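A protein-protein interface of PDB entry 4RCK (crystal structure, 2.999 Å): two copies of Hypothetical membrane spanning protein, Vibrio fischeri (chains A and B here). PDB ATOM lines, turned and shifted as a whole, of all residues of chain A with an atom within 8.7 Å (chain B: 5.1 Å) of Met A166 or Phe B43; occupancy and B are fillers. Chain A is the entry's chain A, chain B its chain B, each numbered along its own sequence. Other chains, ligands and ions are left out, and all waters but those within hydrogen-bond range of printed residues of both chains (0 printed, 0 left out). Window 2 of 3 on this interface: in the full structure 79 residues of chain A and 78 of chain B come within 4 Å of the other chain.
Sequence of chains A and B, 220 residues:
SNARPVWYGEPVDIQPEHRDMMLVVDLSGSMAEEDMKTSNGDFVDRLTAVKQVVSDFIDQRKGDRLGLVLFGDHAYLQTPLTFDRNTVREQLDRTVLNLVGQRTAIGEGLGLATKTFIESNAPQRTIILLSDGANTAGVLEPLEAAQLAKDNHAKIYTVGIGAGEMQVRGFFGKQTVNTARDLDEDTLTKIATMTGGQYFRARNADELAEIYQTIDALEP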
ATOM      1  N   GLY A 162      -8.767 -11.232  15.279  1.00  0.00           N
ATOM      2  CA  GLY A 162      -7.602 -10.799  16.028  1.00  0.00           C
ATOM      3  C   GLY A 162      -7.040 -11.953  16.838  1.00  0.00           C
ATOM      4  O   GLY A 162      -7.785 -12.821  17.294  1.00  0.00           O
ATOM      5  N   ALA A 163      -5.725 -11.962  17.024  1.00  0.00           N
ATOM      6  CA  ALA A 163      -5.061 -13.058  17.719  1.00  0.00           C
ATOM      7  C   ALA A 163      -5.256 -12.986  19.229  1.00  0.00           C
ATOM      8  O   ALA A 163      -5.433 -14.010  19.890  1.00  0.00           O
ATOM      9  CB  ALA A 163      -3.577 -13.070  17.385  1.00  0.00           C
ATOM     10  N   GLY A 164      -5.225 -11.774  19.772  1.00  0.00           N
ATOM     11  CA  GLY A 164      -5.239 -11.588  21.210  1.00  0.00           C
ATOM     12  C   GLY A 164      -3.817 -11.607  21.737  1.00  0.00           C
ATOM     13  O   GLY A 164      -2.895 -11.172  21.046  1.00  0.00           O
ATOM     14  N   GLU A 165      -3.636 -12.111  22.954  1.00  0.00           N
ATOM     15  CA  GLU A 165      -2.310 -12.179  23.562  1.00  0.00           C
ATOM     16  C   GLU A 165      -1.367 -13.038  22.725  1.00  0.00           C
ATOM     17  O   GLU A 165      -1.686 -14.175  22.378  1.00  0.00           O
ATOM     18  CB  GLU A 165      -2.395 -12.722  24.991  1.00  0.00           C
ATOM     19  CG  GLU A 165      -1.739 -11.820  26.027  1.00  0.00           C
ATOM     20  CD  GLU A 165      -1.685 -12.445  27.410  1.00  0.00           C
ATOM     21  OE1 GLU A 165      -2.403 -13.438  27.647  1.00  0.00           O
ATOM     22  OE2 GLU A 165      -0.917 -11.943  28.257  1.00  0.00           O
ATOM     23  N   MET A 166      -0.204 -12.481  22.401  1.00  0.00           N
ATOM     24  CA  MET A 166       0.747 -13.145  21.517  1.00  0.00           C
ATOM     25  C   MET A 166       2.183 -12.893  21.971  1.00  0.00           C
ATOM     26  O   MET A 166       2.586 -11.747  22.173  1.00  0.00           O
ATOM     27  CB  MET A 166       0.555 -12.662  20.075  1.00  0.00           C
ATOM     28  CG  MET A 166       0.635 -13.755  19.022  1.00  0.00           C
ATOM     29  SD  MET A 166       0.141 -13.118  17.241  1.00  0.00           S
ATOM     30  CE  MET A 166       1.576 -11.828  16.961  1.00  0.00           C
ATOM     31  N   GLN A 167       2.944 -13.970  22.140  1.00  0.00           N
ATOM     32  CA  GLN A 167       4.366 -13.870  22.457  1.00  0.00           C
ATOM     33  C   GLN A 167       5.152 -13.603  21.183  1.00  0.00           C
ATOM     34  O   GLN A 167       4.968 -14.285  20.175  1.00  0.00           O
ATOM     35  CB  GLN A 167       4.865 -15.146  23.142  1.00  0.00           C
ATOM     36  CG  GLN A 167       6.346 -15.460  22.926  1.00  0.00           C
ATOM     37  CD  GLN A 167       7.274 -14.598  23.764  1.00  0.00           C
ATOM     38  OE1 GLN A 167       7.680 -13.514  23.347  1.00  0.00           O
ATOM     39  NE2 GLN A 167       7.623 -15.085  24.950  1.00  0.00           N
ATOM     40  N   VAL A 168       6.026 -12.605  21.229  1.00  0.00           N
ATOM     41  CA  VAL A 168       6.752 -12.194  20.040  1.00  0.00           C
ATOM     42  C   VAL A 168       8.206 -11.872  20.375  1.00  0.00           C
ATOM     43  O   VAL A 168       8.522 -11.431  21.482  1.00  0.00           O
ATOM     44  CB  VAL A 168       6.061 -10.975  19.366  1.00  0.00           C
ATOM     45  CG1 VAL A 168       6.917  -9.715  19.462  1.00  0.00           C
ATOM     46  CG2 VAL A 168       5.714 -11.290  17.916  1.00  0.00           C
ATOM     47  N   ARG A 169       9.088 -12.128  19.415  1.00  0.00           N
ATOM     48  CA  ARG A 169      10.494 -11.790  19.553  1.00  0.00           C
ATOM     49  C   ARG A 169      10.784 -10.455  18.896  1.00  0.00           C
ATOM     50  O   ARG A 169      11.007 -10.393  17.685  1.00  0.00           O
ATOM     51  CB  ARG A 169      11.369 -12.866  18.920  1.00  0.00           C
ATOM     52  CG  ARG A 169      12.836 -12.761  19.267  1.00  0.00           C
ATOM     53  CD  ARG A 169      13.221 -13.914  20.161  1.00  0.00           C
ATOM     54  NE  ARG A 169      12.654 -15.152  19.644  1.00  0.00           N
ATOM     55  CZ  ARG A 169      13.126 -16.362  19.911  1.00  0.00           C
ATOM     56  NH1 ARG A 169      12.542 -17.433  19.391  1.00  0.00           N
ATOM     57  NH2 ARG A 169      14.186 -16.505  20.695  1.00  0.00           N
ATOM     58  N   LYS A 174      12.132 -10.540  23.818  1.00  0.00           N
ATOM     59  CA  LYS A 174      10.835 -11.206  23.805  1.00  0.00           C
ATOM     60  C   LYS A 174       9.773 -10.316  24.442  1.00  0.00           C
ATOM     61  O   LYS A 174      10.015  -9.690  25.473  1.00  0.00           O
ATOM     62  CB  LYS A 174      10.926 -12.554  24.518  1.00  0.00           C
ATOM     63  CG  LYS A 174      11.886 -13.515  23.835  1.00  0.00           C
ATOM     64  CD  LYS A 174      12.465 -14.518  24.812  1.00  0.00           C
ATOM     65  CE  LYS A 174      11.409 -15.493  25.300  1.00  0.00           C
ATOM     66  NZ  LYS A 174      10.938 -16.393  24.210  1.00  0.00           N
ATOM     67  N   GLN A 175       8.601 -10.261  23.817  1.00  0.00           N
ATOM     68  CA  GLN A 175       7.575  -9.298  24.200  1.00  0.00           C
ATOM     69  C   GLN A 175       6.170  -9.881  24.070  1.00  0.00           C
ATOM     70  O   GLN A 175       5.902 -10.687  23.180  1.00  0.00           O
ATOM     71  CB  GLN A 175       7.713  -8.033  23.344  1.00  0.00           C
ATOM     72  CG  GLN A 175       6.751  -6.902  23.686  1.00  0.00           C
ATOM     73  CD  GLN A 175       7.046  -5.642  22.909  1.00  0.00           C
ATOM     74  OE1 GLN A 175       8.133  -5.490  22.349  1.00  0.00           O
ATOM     75  NE2 GLN A 175       6.077  -4.727  22.865  1.00  0.00           N
ATOM     76  N   THR A 176       5.283  -9.477  24.974  1.00  0.00           N
ATOM     77  CA  THR A 176       3.901  -9.933  24.943  1.00  0.00           C
ATOM     78  C   THR A 176       2.964  -8.872  24.374  1.00  0.00           C
ATOM     79  O   THR A 176       2.725  -7.836  24.994  1.00  0.00           O
ATOM     80  CB  THR A 176       3.411 -10.331  26.342  1.00  0.00           C
ATOM     81  OG1 THR A 176       4.183 -11.441  26.818  1.00  0.00           O
ATOM     82  CG2 THR A 176       1.945 -10.726  26.293  1.00  0.00           C
ATOM     83  N   VAL A 177       2.432  -9.147  23.189  1.00  0.00           N
ATOM     84  CA  VAL A 177       1.513  -8.233  22.525  1.00  0.00           C
ATOM     85  C   VAL A 177       0.098  -8.798  22.512  1.00  0.00           C
ATOM     86  O   VAL A 177      -0.111  -9.953  22.143  1.00  0.00           O
ATOM     87  CB  VAL A 177       1.954  -7.948  21.072  1.00  0.00           C
ATOM     88  CG1 VAL A 177       1.152  -6.798  20.486  1.00  0.00           C
ATOM     89  CG2 VAL A 177       3.444  -7.648  21.018  1.00  0.00           C
ATOM     90  N   ASN A 178      -0.868  -7.990  22.941  1.00  0.00           N
ATOM     91  CA  ASN A 178      -2.277  -8.320  22.751  1.00  0.00           C
ATOM     92  C   ASN A 178      -2.799  -7.544  21.552  1.00  0.00           C
ATOM     93  O   ASN A 178      -3.050  -6.341  21.641  1.00  0.00           O
ATOM     94  CB  ASN A 178      -3.100  -8.012  24.004  1.00  0.00           C
ATOM     95  CG  ASN A 178      -4.561  -8.404  23.854  1.00  0.00           C
ATOM     96  OD1 ASN A 178      -4.896  -9.587  23.793  1.00  0.00           O
ATOM     97  ND2 ASN A 178      -5.439  -7.407  23.804  1.00  0.00           N
ATOM     98  N   THR A 179      -2.959  -8.242  20.433  1.00  0.00           N
ATOM     99  CA  THR A 179      -3.171  -7.596  19.141  1.00  0.00           C
ATOM    100  C   THR A 179      -4.595  -7.107  18.884  1.00  0.00           C
ATOM    101  O   THR A 179      -4.831  -6.352  17.939  1.00  0.00           O
ATOM    102  CB  THR A 179      -2.783  -8.541  18.004  1.00  0.00           C
ATOM    103  OG1 THR A 179      -3.590  -9.722  18.070  1.00  0.00           O
ATOM    104  CG2 THR A 179      -1.320  -8.936  18.118  1.00  0.00           C
ATOM    105  N   ALA A 180      -5.536  -7.529  19.721  1.00  0.00           N
ATOM    106  CA  ALA A 180      -6.919  -7.096  19.574  1.00  0.00           C
ATOM    107  C   ALA A 180      -7.459  -6.519  20.873  1.00  0.00           C
ATOM    108  O   ALA A 180      -8.414  -7.044  21.445  1.00  0.00           O
ATOM    109  CB  ALA A 180      -7.793  -8.250  19.102  1.00  0.00           C
ATOM    110  N   ARG A 203      -9.110 -16.268  15.870  1.00  0.00           N
ATOM    111  CA  ARG A 203      -7.801 -15.936  16.420  1.00  0.00           C
ATOM    112  C   ARG A 203      -6.672 -16.300  15.460  1.00  0.00           C
ATOM    113  O   ARG A 203      -5.508 -15.987  15.712  1.00  0.00           O
ATOM    114  CB  ARG A 203      -7.601 -16.625  17.770  1.00  0.00           C
ATOM    115  CG  ARG A 203      -8.343 -15.935  18.904  1.00  0.00           C
ATOM    116  CD  ARG A 203      -8.072 -16.588  20.247  1.00  0.00           C
ATOM    117  NE  ARG A 203      -8.648 -15.815  21.343  1.00  0.00           N
ATOM    118  CZ  ARG A 203      -9.916 -15.901  21.734  1.00  0.00           C
ATOM    119  NH1 ARG A 203     -10.748 -16.730  21.117  1.00  0.00           N
ATOM    120  NH2 ARG A 203     -10.354 -15.156  22.740  1.00  0.00           N
ATOM    121  N   ASN A 204      -7.027 -16.957  14.359  1.00  0.00           N
ATOM    122  CA  ASN A 204      -6.083 -17.205  13.274  1.00  0.00           C
ATOM    123  C   ASN A 204      -6.810 -17.512  11.967  1.00  0.00           C
ATOM    124  O   ASN A 204      -8.042 -17.515  11.917  1.00  0.00           O
ATOM    125  CB  ASN A 204      -5.123 -18.343  13.631  1.00  0.00           C
ATOM    126  CG  ASN A 204      -5.819 -19.680  13.754  1.00  0.00           C
ATOM    127  OD1 ASN A 204      -6.061 -20.358  12.758  1.00  0.00           O
ATOM    128  ND2 ASN A 204      -6.132 -20.076  14.982  1.00  0.00           N
ATOM    129  N   ALA A 205      -6.041 -17.766  10.912  1.00  0.00           N
ATOM    130  CA  ALA A 205      -6.593 -17.946   9.572  1.00  0.00           C
ATOM    131  C   ALA A 205      -7.420 -19.221   9.441  1.00  0.00           C
ATOM    132  O   ALA A 205      -8.338 -19.293   8.621  1.00  0.00           O
ATOM    133  CB  ALA A 205      -5.472 -17.943   8.543  1.00  0.00           C
ATOM    134  N   GLU B  34      -0.287  -7.972  10.941  1.00  0.00           N
ATOM    135  CA  GLU B  34      -0.030  -9.357  10.581  1.00  0.00           C
ATOM    136  C   GLU B  34      -0.291 -10.241  11.783  1.00  0.00           C
ATOM    137  O   GLU B  34       0.616 -10.629  12.514  1.00  0.00           O
ATOM    138  CB  GLU B  34       1.391  -9.519  10.045  1.00  0.00           C
ATOM    139  CG  GLU B  34       1.476  -9.100   8.587  1.00  0.00           C
ATOM    140  CD  GLU B  34       2.882  -8.799   8.129  1.00  0.00           C
ATOM    141  OE1 GLU B  34       3.618  -8.092   8.850  1.00  0.00           O
ATOM    142  OE2 GLU B  34       3.245  -9.251   7.025  1.00  0.00           O
ATOM    143  N   ASP B  35      -1.571 -10.538  11.958  1.00  0.00           N
ATOM    144  CA  ASP B  35      -2.088 -11.266  13.096  1.00  0.00           C
ATOM    145  C   ASP B  35      -2.154 -12.753  12.802  1.00  0.00           C
ATOM    146  O   ASP B  35      -1.771 -13.595  13.620  1.00  0.00           O
ATOM    147  CB  ASP B  35      -3.489 -10.750  13.436  1.00  0.00           C
ATOM    148  CG  ASP B  35      -3.578 -10.169  14.823  1.00  0.00           C
ATOM    149  OD1 ASP B  35      -2.727 -10.524  15.661  1.00  0.00           O
ATOM    150  OD2 ASP B  35      -4.503  -9.364  15.074  1.00  0.00           O
ATOM    151  N   MET B  36      -2.624 -13.051  11.597  1.00  0.00           N
ATOM    152  CA  MET B  36      -3.219 -14.340  11.293  1.00  0.00           C
ATOM    153  C   MET B  36      -2.235 -15.451  10.961  1.00  0.00           C
ATOM    154  O   MET B  36      -1.433 -15.357  10.033  1.00  0.00           O
ATOM    155  CB  MET B  36      -4.220 -14.159  10.157  1.00  0.00           C
ATOM    156  CG  MET B  36      -5.325 -13.161  10.496  1.00  0.00           C
ATOM    157  SD  MET B  36      -6.660 -13.844  11.760  1.00  0.00           S
ATOM    158  CE  MET B  36      -5.774 -13.514  13.471  1.00  0.00           C
ATOM    159  N   LYS B  37      -2.348 -16.516  11.743  1.00  0.00           N
ATOM    160  CA  LYS B  37      -1.488 -17.683  11.659  1.00  0.00           C
ATOM    161  C   LYS B  37      -2.100 -18.754  10.762  1.00  0.00           C
ATOM    162  O   LYS B  37      -3.236 -19.174  10.977  1.00  0.00           O
ATOM    163  CB  LYS B  37      -1.252 -18.240  13.064  1.00  0.00           C
ATOM    164  CG  LYS B  37      -0.314 -19.417  13.137  1.00  0.00           C
ATOM    165  CD  LYS B  37       1.126 -18.961  13.070  1.00  0.00           C
ATOM    166  CE  LYS B  37       2.023 -19.881  13.878  1.00  0.00           C
ATOM    167  NZ  LYS B  37       3.462 -19.620  13.605  1.00  0.00           N
ATOM    168  N   GLY B  41       2.301 -22.246   9.645  1.00  0.00           N
ATOM    169  CA  GLY B  41       2.849 -21.449  10.727  1.00  0.00           C
ATOM    170  C   GLY B  41       3.231 -20.022  10.382  1.00  0.00           C
ATOM    171  O   GLY B  41       3.768 -19.302  11.224  1.00  0.00           O
ATOM    172  N   ASP B  42       2.963 -19.603   9.151  1.00  0.00           N
ATOM    173  CA  ASP B  42       3.315 -18.254   8.727  1.00  0.00           C
ATOM    174  C   ASP B  42       2.309 -17.230   9.244  1.00  0.00           C
ATOM    175  O   ASP B  42       1.168 -17.569   9.559  1.00  0.00           O
ATOM    176  CB  ASP B  42       3.410 -18.178   7.200  1.00  0.00           C
ATOM    177  CG  ASP B  42       3.895 -16.824   6.712  1.00  0.00           C
ATOM    178  OD1 ASP B  42       4.705 -16.190   7.422  1.00  0.00           O
ATOM    179  OD2 ASP B  42       3.459 -16.389   5.625  1.00  0.00           O
ATOM    180  N   PHE B  43       2.745 -15.977   9.339  1.00  0.00           N
ATOM    181  CA  PHE B  43       1.860 -14.878   9.697  1.00  0.00           C
ATOM    182  C   PHE B  43       1.594 -13.986   8.491  1.00  0.00           C
ATOM    183  O   PHE B  43       2.518 -13.595   7.776  1.00  0.00           O
ATOM    184  CB  PHE B  43       2.452 -14.050  10.840  1.00  0.00           C
ATOM    185  CG  PHE B  43       2.369 -14.719  12.181  1.00  0.00           C
ATOM    186  CD1 PHE B  43       1.236 -14.584  12.967  1.00  0.00           C
ATOM    187  CD2 PHE B  43       3.423 -15.477  12.659  1.00  0.00           C
ATOM    188  CE1 PHE B  43       1.155 -15.197  14.204  1.00  0.00           C
ATOM    189  CE2 PHE B  43       3.348 -16.093  13.895  1.00  0.00           C
ATOM    190  CZ  PHE B  43       2.212 -15.952  14.668  1.00  0.00           C
ATOM    191  N   VAL B  44       0.324 -13.678   8.265  1.00  0.00           N
ATOM    192  CA  VAL B  44      -0.064 -12.752   7.212  1.00  0.00           C
ATOM    193  C   VAL B  44      -1.041 -11.740   7.801  1.00  0.00           C
ATOM    194  O   VAL B  44      -1.595 -11.962   8.879  1.00  0.00           O
ATOM    195  CB  VAL B  44      -0.693 -13.485   6.006  1.00  0.00           C
ATOM    196  CG1 VAL B  44      -2.180 -13.737   6.239  1.00  0.00           C
ATOM    197  CG2 VAL B  44      -0.467 -12.693   4.727  1.00  0.00           C
ATOM    198  N   ASP B  45      -1.243 -10.626   7.108  1.00  0.00           N
ATOM    199  CA  ASP B  45      -2.102  -9.567   7.625  1.00  0.00           C
ATOM    200  C   ASP B  45      -3.571  -9.973   7.592  1.00  0.00           C
ATOM    201  O   ASP B  45      -3.958 -10.893   6.870  1.00  0.00           O
ATOM    202  CB  ASP B  45      -1.891  -8.273   6.840  1.00  0.00           C
ATOM    203  CG  ASP B  45      -2.205  -8.428   5.370  1.00  0.00           C
ATOM    204  OD1 ASP B  45      -1.409  -9.074   4.655  1.00  0.00           O
ATOM    205  OD2 ASP B  45      -3.245  -7.899   4.926  1.00  0.00           O
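No position is printed for both chains.
The side-chain carboxylate (OD2) of Asp B35 is in hydrogen-bond range of the backbone NH (N) of Ala A163 (3.5 Å).
The side-chain hydroxyl (OG1) of Thr A179 sits at hydrogen-bond distance from the side-chain carboxylate (OD1) of Asp B35 (2.7 Å).
N of Ala A205 sits at hydrogen-bond distance from O of Lys B37 (3.1 Å).
Among the printed residues, pairs that only touch across the chains: Gly A162 with Asp B35 (3.5 Å), Gly A162 with Met B36 (3.9 Å), Ala A163 with Met B36 (3.9 Å), Met A166 with Phe B43 (3.8 Å), Arg A203 with Met B36 (3.3 Å), Asn A204 with Met B36 (3.7 Å) and Asn A204 with Lys B37 (3.4 Å).
N of Ala A163 sits at hydrogen-bond distance from OG1 of Thr A179, 3.3 Å away.
N of Thr A179 lies within hydrogen-bond range of O of Gly A164, at 3.0 Å.
The backbone NH of Met A166 is in hydrogen-bond range of the backbone carbonyl oxygen of Val A177 (2.5 Å).
The backbone NH (N) of Asp B35 sits at hydrogen-bond distance from the backbone carbonyl oxygen (O) of Val B44, 3.4 Å away.
The backbone NH of Val B44 sits at hydrogen-bond distance from the backbone carbonyl oxygen of Met B36, at 3.0 Å.
The backbone carbonyl oxygen (O) of Gly B41 lies within hydrogen-bond range of the side-chain amino group (NZ) of Lys B37 (2.4 Å).
Hydrophobic or aromatic side chains of chain A within 4 Å of the printed part of chain B: Ala A163, Met A166 and Ala A205.
Printed residues of chain B that touch a printed residue of chain A: Asp B35, Met B36, Lys B37 and Phe B43.
Hydrophobic or aromatic side chains of chain B that line the printed part of chain A: Met B36 and Phe B43.
Along chain B the printed residues that touch a printed residue of chain A span positions 35 to 43.
Among the printed residues, 10 pairs touch across the chains.
Of chain B, only Phe B43 comes within 4 Å of Met A166.
Of chain A, only Met A166 comes within 4 Å of Phe B43.
No residue of chain A comes within 4 Å of Asp B42.
No residue of chain A comes within 4 Å of Val B44.
Of the printed residues of chain B, Thr A179 touches Asp B35 (2.7 Å).
Of the printed residues of chain A, Lys B37 touches Asn A204 and Ala A205.
Printed residues of chain B within 4 Å of Arg A203: Met B36 (3.3 Å).
Of the printed residues of chain B, Gly A162 touches Asp B35 and Met B36.
Of the printed residues of chain B, Asn A204 touches Met B36 and Lys B37.
Val A168 touches none of the printed residues of chain B.
The nearest residue of chain A that does not touch Phe B43 is Ala A163 (6.1 Å).
The nearest printed residue of chain A that does not touch Asp B35 is Met A166 (4.1 Å).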
